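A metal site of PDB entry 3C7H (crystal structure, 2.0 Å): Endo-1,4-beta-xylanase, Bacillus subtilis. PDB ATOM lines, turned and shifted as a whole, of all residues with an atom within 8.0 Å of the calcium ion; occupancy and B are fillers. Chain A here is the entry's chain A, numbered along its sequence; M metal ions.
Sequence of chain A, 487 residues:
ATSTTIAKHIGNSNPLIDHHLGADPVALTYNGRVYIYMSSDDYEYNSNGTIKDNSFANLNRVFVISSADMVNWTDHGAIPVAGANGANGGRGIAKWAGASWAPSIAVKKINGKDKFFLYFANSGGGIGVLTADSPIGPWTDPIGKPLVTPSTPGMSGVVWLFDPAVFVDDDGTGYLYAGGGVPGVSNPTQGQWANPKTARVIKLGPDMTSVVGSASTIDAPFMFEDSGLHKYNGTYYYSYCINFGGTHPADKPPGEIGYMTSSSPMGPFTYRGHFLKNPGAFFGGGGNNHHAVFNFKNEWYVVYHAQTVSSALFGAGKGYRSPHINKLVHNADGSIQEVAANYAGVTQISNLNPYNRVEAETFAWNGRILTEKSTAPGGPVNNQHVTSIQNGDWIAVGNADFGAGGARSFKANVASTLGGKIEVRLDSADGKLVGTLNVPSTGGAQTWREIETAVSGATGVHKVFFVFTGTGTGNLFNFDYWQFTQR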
ATOM      1  N   THR A  74     -36.399  11.726   9.638  1.00  0.00           N
ATOM      2  CA  THR A  74     -35.145  11.515  10.380  1.00  0.00           C
ATOM      3  C   THR A  74     -34.524  10.246   9.863  1.00  0.00           C
ATOM      4  O   THR A  74     -35.160   9.185   9.816  1.00  0.00           O
ATOM      5  CB  THR A  74     -35.400  11.341  11.917  1.00  0.00           C
ATOM      6  OG1 THR A  74     -36.116  12.481  12.407  1.00  0.00           O
ATOM      7  CG2 THR A  74     -34.092  11.216  12.697  1.00  0.00           C
ATOM      8  N   ASP A  75     -33.285  10.369   9.415  1.00  0.00           N
ATOM      9  CA  ASP A  75     -32.552   9.231   8.930  1.00  0.00           C
ATOM     10  C   ASP A  75     -31.816   8.586  10.109  1.00  0.00           C
ATOM     11  O   ASP A  75     -30.969   9.222  10.746  1.00  0.00           O
ATOM     12  CB  ASP A  75     -31.576   9.641   7.813  1.00  0.00           C
ATOM     13  CG  ASP A  75     -31.162   8.449   6.963  1.00  0.00           C
ATOM     14  OD1 ASP A  75     -30.684   7.457   7.563  1.00  0.00           O
ATOM     15  OD2 ASP A  75     -31.311   8.538   5.733  1.00  0.00           O
ATOM     16  N   ARG A 357     -33.797  20.542  19.887  1.00  0.00           N
ATOM     17  CA  ARG A 357     -32.764  19.984  19.035  1.00  0.00           C
ATOM     18  C   ARG A 357     -33.462  19.168  17.939  1.00  0.00           C
ATOM     19  O   ARG A 357     -34.328  18.324  18.224  1.00  0.00           O
ATOM     20  CB  ARG A 357     -31.806  19.086  19.827  1.00  0.00           C
ATOM     21  CG  ARG A 357     -30.976  18.090  18.970  1.00  0.00           C
ATOM     22  CD  ARG A 357     -29.897  17.333  19.800  1.00  0.00           C
ATOM     23  NE  ARG A 357     -29.218  16.382  18.932  1.00  0.00           N
ATOM     24  CZ  ARG A 357     -27.977  15.958  19.088  1.00  0.00           C
ATOM     25  NH1 ARG A 357     -27.242  16.391  20.118  1.00  0.00           N
ATOM     26  NH2 ARG A 357     -27.448  15.094  18.210  1.00  0.00           N
ATOM     27  N   VAL A 358     -33.143  19.512  16.683  1.00  0.00           N
ATOM     28  CA  VAL A 358     -33.596  18.789  15.495  1.00  0.00           C
ATOM     29  C   VAL A 358     -32.319  18.263  14.800  1.00  0.00           C
ATOM     30  O   VAL A 358     -31.377  19.024  14.546  1.00  0.00           O
ATOM     31  CB  VAL A 358     -34.416  19.699  14.521  1.00  0.00           C
ATOM     32  CG1 VAL A 358     -34.858  18.919  13.268  1.00  0.00           C
ATOM     33  CG2 VAL A 358     -35.632  20.334  15.225  1.00  0.00           C
ATOM     34  N   GLU A 359     -32.271  16.965  14.540  1.00  0.00           N
ATOM     35  CA  GLU A 359     -31.138  16.389  13.803  1.00  0.00           C
ATOM     36  C   GLU A 359     -31.001  17.073  12.440  1.00  0.00           C
ATOM     37  O   GLU A 359     -32.002  17.328  11.808  1.00  0.00           O
ATOM     38  CB  GLU A 359     -31.351  14.880  13.627  1.00  0.00           C
ATOM     39  CG  GLU A 359     -31.373  14.103  14.926  1.00  0.00           C
ATOM     40  CD  GLU A 359     -30.247  14.505  15.884  1.00  0.00           C
ATOM     41  OE1 GLU A 359     -29.086  14.661  15.450  1.00  0.00           O
ATOM     42  OE2 GLU A 359     -30.543  14.659  17.085  1.00  0.00           O
ATOM     43  N   ALA A 360     -29.766  17.354  11.986  1.00  0.00           N
ATOM     44  CA  ALA A 360     -29.592  17.885  10.640  1.00  0.00           C
ATOM     45  C   ALA A 360     -30.139  16.876   9.602  1.00  0.00           C
ATOM     46  O   ALA A 360     -30.647  17.273   8.569  1.00  0.00           O
ATOM     47  CB  ALA A 360     -28.129  18.209  10.366  1.00  0.00           C
ATOM     48  N   GLU A 361     -30.073  15.589   9.965  1.00  0.00           N
ATOM     49  CA  GLU A 361     -30.550  14.466   9.139  1.00  0.00           C
ATOM     50  C   GLU A 361     -32.063  14.258   9.270  1.00  0.00           C
ATOM     51  O   GLU A 361     -32.615  13.239   8.803  1.00  0.00           O
ATOM     52  CB  GLU A 361     -29.792  13.174   9.477  1.00  0.00           C
ATOM     53  CG  GLU A 361     -30.082  12.617  10.905  1.00  0.00           C
ATOM     54  CD  GLU A 361     -29.091  13.059  11.956  1.00  0.00           C
ATOM     55  OE1 GLU A 361     -28.410  14.137  11.805  1.00  0.00           O
ATOM     56  OE2 GLU A 361     -28.996  12.322  12.976  1.00  0.00           O
ATOM     57  N   THR A 362     -32.731  15.221   9.897  1.00  0.00           N
ATOM     58  CA  THR A 362     -34.184  15.370   9.815  1.00  0.00           C
ATOM     59  C   THR A 362     -34.541  16.458   8.794  1.00  0.00           C
ATOM     60  O   THR A 362     -34.451  17.654   9.071  1.00  0.00           O
ATOM     61  CB  THR A 362     -34.842  15.697  11.195  1.00  0.00           C
ATOM     62  OG1 THR A 362     -34.595  14.630  12.115  1.00  0.00           O
ATOM     63  CG2 THR A 362     -36.381  15.919  11.045  1.00  0.00           C
ATOM     64  N   GLU A 372     -24.652   9.900   6.978  1.00  0.00           N
ATOM     65  CA  GLU A 372     -23.877   8.737   7.428  1.00  0.00           C
ATOM     66  C   GLU A 372     -23.785   8.759   8.947  1.00  0.00           C
ATOM     67  O   GLU A 372     -24.147   9.744   9.566  1.00  0.00           O
ATOM     68  CB  GLU A 372     -22.464   8.792   6.818  1.00  0.00           C
ATOM     69  CG  GLU A 372     -21.556   9.817   7.449  1.00  0.00           C
ATOM     70  CD  GLU A 372     -20.183   9.923   6.753  1.00  0.00           C
ATOM     71  OE1 GLU A 372     -19.930   9.118   5.842  1.00  0.00           O
ATOM     72  OE2 GLU A 372     -19.378  10.825   7.102  1.00  0.00           O
ATOM     73  N   LYS A 373     -23.244   7.690   9.537  1.00  0.00           N
ATOM     74  CA  LYS A 373     -23.105   7.635  10.986  1.00  0.00           C
ATOM     75  C   LYS A 373     -22.106   8.681  11.425  1.00  0.00           C
ATOM     76  O   LYS A 373     -21.068   8.834  10.792  1.00  0.00           O
ATOM     77  CB  LYS A 373     -22.636   6.248  11.419  1.00  0.00           C
ATOM     78  CG  LYS A 373     -22.698   6.003  12.930  1.00  0.00           C
ATOM     79  CD  LYS A 373     -22.303   4.559  13.227  1.00  0.00           C
ATOM     80  CE  LYS A 373     -21.941   4.348  14.683  1.00  0.00           C
ATOM     81  NZ  LYS A 373     -23.030   4.765  15.639  1.00  0.00           N
ATOM     82  N   SER A 374     -22.409   9.377  12.516  1.00  0.00           N
ATOM     83  CA  SER A 374     -21.613  10.529  12.945  1.00  0.00           C
ATOM     84  C   SER A 374     -20.644  10.209  14.072  1.00  0.00           C
ATOM     85  O   SER A 374     -20.959   9.406  14.970  1.00  0.00           O
ATOM     86  CB  SER A 374     -22.525  11.650  13.420  1.00  0.00           C
ATOM     87  OG  SER A 374     -21.780  12.814  13.721  1.00  0.00           O
ATOM     88  N   ALA A 376     -19.944  12.659  16.100  1.00  0.00           N
ATOM     89  CA  ALA A 376     -20.295  13.708  17.064  1.00  0.00           C
ATOM     90  C   ALA A 376     -20.582  13.142  18.450  1.00  0.00           C
ATOM     91  O   ALA A 376     -21.342  12.187  18.562  1.00  0.00           O
ATOM     92  CB  ALA A 376     -21.483  14.518  16.572  1.00  0.00           C
ATOM     93  N   GLY A 378     -22.332  12.534  22.008  1.00  0.00           N
ATOM     94  CA  GLY A 378     -23.752  12.542  22.391  1.00  0.00           C
ATOM     95  C   GLY A 378     -24.664  12.147  21.231  1.00  0.00           C
ATOM     96  O   GLY A 378     -24.283  11.344  20.380  1.00  0.00           O
ATOM     97  N   GLY A 379     -25.863  12.714  21.177  1.00  0.00           N
ATOM     98  CA  GLY A 379     -26.784  12.437  20.066  1.00  0.00           C
ATOM     99  C   GLY A 379     -27.633  11.202  20.346  1.00  0.00           C
ATOM    100  O   GLY A 379     -27.334  10.426  21.254  1.00  0.00           O
ATOM    101  N   PRO A 380     -28.707  11.006  19.547  1.00  0.00           N
ATOM    102  CA  PRO A 380     -29.595   9.839  19.694  1.00  0.00           C
ATOM    103  C   PRO A 380     -28.889   8.536  19.290  1.00  0.00           C
ATOM    104  O   PRO A 380     -27.775   8.577  18.716  1.00  0.00           O
ATOM    105  CB  PRO A 380     -30.729  10.136  18.683  1.00  0.00           C
ATOM    106  CG  PRO A 380     -30.102  11.047  17.648  1.00  0.00           C
ATOM    107  CD  PRO A 380     -29.121  11.905  18.449  1.00  0.00           C
ATOM    108  N   ASN A 382     -27.576   5.621  17.208  1.00  0.00           N
ATOM    109  CA  ASN A 382     -27.166   5.544  15.795  1.00  0.00           C
ATOM    110  C   ASN A 382     -27.151   6.921  15.130  1.00  0.00           C
ATOM    111  O   ASN A 382     -27.390   7.030  13.921  1.00  0.00           O
ATOM    112  CB  ASN A 382     -28.016   4.534  14.983  1.00  0.00           C
ATOM    113  CG  ASN A 382     -27.180   3.791  13.923  1.00  0.00           C
ATOM    114  OD1 ASN A 382     -26.021   3.464  14.154  1.00  0.00           O
ATOM    115  ND2 ASN A 382     -27.777   3.513  12.762  1.00  0.00           N
ATOM    116  N   ASN A 383     -26.910   7.969  15.925  1.00  0.00           N
ATOM    117  CA  ASN A 383     -26.804   9.361  15.422  1.00  0.00           C
ATOM    118  C   ASN A 383     -26.048   9.459  14.092  1.00  0.00           C
ATOM    119  O   ASN A 383     -24.946   8.876  13.910  1.00  0.00           O
ATOM    120  CB  ASN A 383     -26.152  10.261  16.489  1.00  0.00           C
ATOM    121  CG  ASN A 383     -26.118  11.746  16.070  1.00  0.00           C
ATOM    122  OD1 ASN A 383     -27.102  12.278  15.535  1.00  0.00           O
ATOM    123  ND2 ASN A 383     -24.983  12.395  16.280  1.00  0.00           N
ATOM    124  N   GLN A 384     -26.650  10.161  13.150  1.00  0.00           N
ATOM    125  CA  GLN A 384     -26.090  10.385  11.833  1.00  0.00           C
ATOM    126  C   GLN A 384     -25.718  11.864  11.693  1.00  0.00           C
ATOM    127  O   GLN A 384     -25.951  12.662  12.599  1.00  0.00           O
ATOM    128  CB  GLN A 384     -27.135  10.019  10.747  1.00  0.00           C
ATOM    129  CG  GLN A 384     -27.713   8.581  10.915  1.00  0.00           C
ATOM    130  CD  GLN A 384     -26.786   7.524  10.366  1.00  0.00           C
ATOM    131  OE1 GLN A 384     -26.507   7.528   9.163  1.00  0.00           O
ATOM    132  NE2 GLN A 384     -26.316   6.612  11.226  1.00  0.00           N
ATOM    133  N   HIS A 385     -25.102  12.211  10.576  1.00  0.00           N
ATOM    134  CA  HIS A 385     -24.915  13.649  10.253  1.00  0.00           C
ATOM    135  C   HIS A 385     -25.091  13.814   8.755  1.00  0.00           C
ATOM    136  O   HIS A 385     -25.084  12.824   8.004  1.00  0.00           O
ATOM    137  CB  HIS A 385     -23.567  14.229  10.761  1.00  0.00           C
ATOM    138  CG  HIS A 385     -22.352  13.571  10.181  1.00  0.00           C
ATOM    139  ND1 HIS A 385     -21.233  13.288  10.936  1.00  0.00           N
ATOM    140  CD2 HIS A 385     -22.057  13.155   8.917  1.00  0.00           C
ATOM    141  CE1 HIS A 385     -20.314  12.719  10.173  1.00  0.00           C
ATOM    142  NE2 HIS A 385     -20.793  12.631   8.942  1.00  0.00           N
ATOM    143  N   VAL A 386     -25.318  15.063   8.341  1.00  0.00           N
ATOM    144  CA  VAL A 386     -25.388  15.410   6.939  1.00  0.00           C
ATOM    145  C   VAL A 386     -23.945  15.666   6.463  1.00  0.00           C
ATOM    146  O   VAL A 386     -23.189  16.379   7.118  1.00  0.00           O
ATOM    147  CB  VAL A 386     -26.328  16.633   6.681  1.00  0.00           C
ATOM    148  CG1 VAL A 386     -26.279  17.023   5.202  1.00  0.00           C
ATOM    149  CG2 VAL A 386     -27.757  16.280   7.070  1.00  0.00           C
ATOM    150  N   ASN A 413     -24.571  22.192  15.239  1.00  0.00           N
ATOM    151  CA  ASN A 413     -23.375  21.427  15.609  1.00  0.00           C
ATOM    152  C   ASN A 413     -22.652  20.986  14.347  1.00  0.00           C
ATOM    153  O   ASN A 413     -23.221  20.263  13.523  1.00  0.00           O
ATOM    154  CB  ASN A 413     -23.734  20.225  16.490  1.00  0.00           C
ATOM    155  CG  ASN A 413     -22.536  19.674  17.257  1.00  0.00           C
ATOM    156  OD1 ASN A 413     -21.707  20.446  17.759  1.00  0.00           O
ATOM    157  ND2 ASN A 413     -22.461  18.337  17.394  1.00  0.00           N
ATOM    158  N   TRP A 448     -15.909  18.571  16.672  1.00  0.00           N
ATOM    159  CA  TRP A 448     -17.230  19.208  16.679  1.00  0.00           C
ATOM    160  C   TRP A 448     -17.332  20.424  17.594  1.00  0.00           C
ATOM    161  O   TRP A 448     -16.852  20.402  18.723  1.00  0.00           O
ATOM    162  CB  TRP A 448     -18.325  18.157  17.058  1.00  0.00           C
ATOM    163  CG  TRP A 448     -18.401  17.049  16.039  1.00  0.00           C
ATOM    164  CD1 TRP A 448     -17.611  15.919  15.985  1.00  0.00           C
ATOM    165  CD2 TRP A 448     -19.276  16.987  14.893  1.00  0.00           C
ATOM    166  NE1 TRP A 448     -17.945  15.171  14.876  1.00  0.00           N
ATOM    167  CE2 TRP A 448     -18.963  15.793  14.201  1.00  0.00           C
ATOM    168  CE3 TRP A 448     -20.280  17.818  14.398  1.00  0.00           C
ATOM    169  CZ2 TRP A 448     -19.630  15.412  13.021  1.00  0.00           C
ATOM    170  CZ3 TRP A 448     -20.925  17.445  13.220  1.00  0.00           C
ATOM    171  CH2 TRP A 448     -20.606  16.242  12.550  1.00  0.00           C
ATOM    172  N   PHE A 479     -22.607  18.202   9.431  1.00  0.00           N
ATOM    173  CA  PHE A 479     -23.675  18.968  10.092  1.00  0.00           C
ATOM    174  C   PHE A 479     -24.540  17.952  10.836  1.00  0.00           C
ATOM    175  O   PHE A 479     -25.180  17.081  10.218  1.00  0.00           O
ATOM    176  CB  PHE A 479     -24.451  19.728   8.982  1.00  0.00           C
ATOM    177  CG  PHE A 479     -25.584  20.614   9.451  1.00  0.00           C
ATOM    178  CD1 PHE A 479     -25.696  21.061  10.762  1.00  0.00           C
ATOM    179  CD2 PHE A 479     -26.541  21.037   8.519  1.00  0.00           C
ATOM    180  CE1 PHE A 479     -26.755  21.883  11.150  1.00  0.00           C
ATOM    181  CE2 PHE A 479     -27.591  21.884   8.888  1.00  0.00           C
ATOM    182  CZ  PHE A 479     -27.721  22.297  10.212  1.00  0.00           C
ATOM    183  N   ASP A 480     -24.548  18.040  12.163  1.00  0.00           N
ATOM    184  CA  ASP A 480     -25.092  16.992  13.048  1.00  0.00           C
ATOM    185  C   ASP A 480     -26.506  17.295  13.538  1.00  0.00           C
ATOM    186  O   ASP A 480     -27.392  16.437  13.447  1.00  0.00           O
ATOM    187  CB  ASP A 480     -24.121  16.730  14.236  1.00  0.00           C
ATOM    188  CG  ASP A 480     -24.707  15.801  15.338  1.00  0.00           C
ATOM    189  OD1 ASP A 480     -25.460  14.848  15.040  1.00  0.00           O
ATOM    190  OD2 ASP A 480     -24.382  16.034  16.524  1.00  0.00           O
ATOM    191  N   TYR A 481     -26.730  18.492  14.055  1.00  0.00           N
ATOM    192  CA  TYR A 481     -28.046  18.885  14.558  1.00  0.00           C
ATOM    193  C   TYR A 481     -28.134  20.416  14.611  1.00  0.00           C
ATOM    194  O   TYR A 481     -27.118  21.103  14.483  1.00  0.00           O
ATOM    195  CB  TYR A 481     -28.315  18.263  15.954  1.00  0.00           C
ATOM    196  CG  TYR A 481     -27.525  18.910  17.107  1.00  0.00           C
ATOM    197  CD1 TYR A 481     -27.900  20.165  17.610  1.00  0.00           C
ATOM    198  CD2 TYR A 481     -26.450  18.266  17.697  1.00  0.00           C
ATOM    199  CE1 TYR A 481     -27.190  20.763  18.639  1.00  0.00           C
ATOM    200  CE2 TYR A 481     -25.731  18.857  18.757  1.00  0.00           C
ATOM    201  CZ  TYR A 481     -26.114  20.108  19.209  1.00  0.00           C
ATOM    202  OH  TYR A 481     -25.442  20.723  20.233  1.00  0.00           O
ATOM    203  N   TRP A 482     -29.333  20.941  14.760  1.00  0.00           N
ATOM    204  CA  TRP A 482     -29.532  22.378  14.911  1.00  0.00           C
ATOM    205  C   TRP A 482     -30.656  22.639  15.895  1.00  0.00           C
ATOM    206  O   TRP A 482     -31.423  21.720  16.266  1.00  0.00           O
ATOM    207  CB  TRP A 482     -29.861  23.060  13.565  1.00  0.00           C
ATOM    208  CG  TRP A 482     -30.966  22.437  12.720  1.00  0.00           C
ATOM    209  CD1 TRP A 482     -30.819  21.527  11.694  1.00  0.00           C
ATOM    210  CD2 TRP A 482     -32.387  22.699  12.804  1.00  0.00           C
ATOM    211  NE1 TRP A 482     -32.034  21.224  11.144  1.00  0.00           N
ATOM    212  CE2 TRP A 482     -33.022  21.916  11.800  1.00  0.00           C
ATOM    213  CE3 TRP A 482     -33.183  23.514  13.622  1.00  0.00           C
ATOM    214  CZ2 TRP A 482     -34.419  21.912  11.602  1.00  0.00           C
ATOM    215  CZ3 TRP A 482     -34.580  23.523  13.420  1.00  0.00           C
ATOM    216  CH2 TRP A 482     -35.174  22.725  12.429  1.00  0.00           C
HETATM  217 CA    CA M   1     -27.374  14.003  13.990  1.00  0.00          CA
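The backbone carbonyl oxygen (O) of Asn 383 lies within hydrogen-bond range of the backbone NH (N) of Ser 374. OD2 of Asp 480 is in salt-bridge range of NH2 of Arg 357, at 3.6 Å. The backbone NH of Ala 360 sits close to the backbone carbonyl oxygen of Asp 480 (2.9 Å). O of Asn 413 is in hydrogen-bond range of N of Asp 480 (2.9 Å). The guanidinium group (NE) of Arg 357 lies within salt-bridge range of the side-chain carboxylate (OE2) of Glu 359, 2.9 Å away. OE1 of Gln 384 lies close to O of Glu 372. The backbone carbonyl oxygen (O) of Asn 382 lies within hydrogen-bond range of the side-chain amide nitrogen (NE2) of Gln 384 (2.9 Å). OE1 of Gln 384 sits at hydrogen-bond distance from N of Lys 373, 3.3 Å away.
The calcium ion is bound by the side-chain amide oxygen (OD1) of Asn 383, the side-chain carboxylate (OD1) of Asp 480, the side-chain carboxylate (OE1) of Glu 359, the backbone carbonyl oxygen (O) of Gln 384, the side-chain carboxylate (OE1) of Glu 361, the backbone carbonyl oxygen (O) of Asp 480 and the side-chain carboxylate (OE2) of Glu 361. The calcium ion has seven donor atoms within binding distance.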
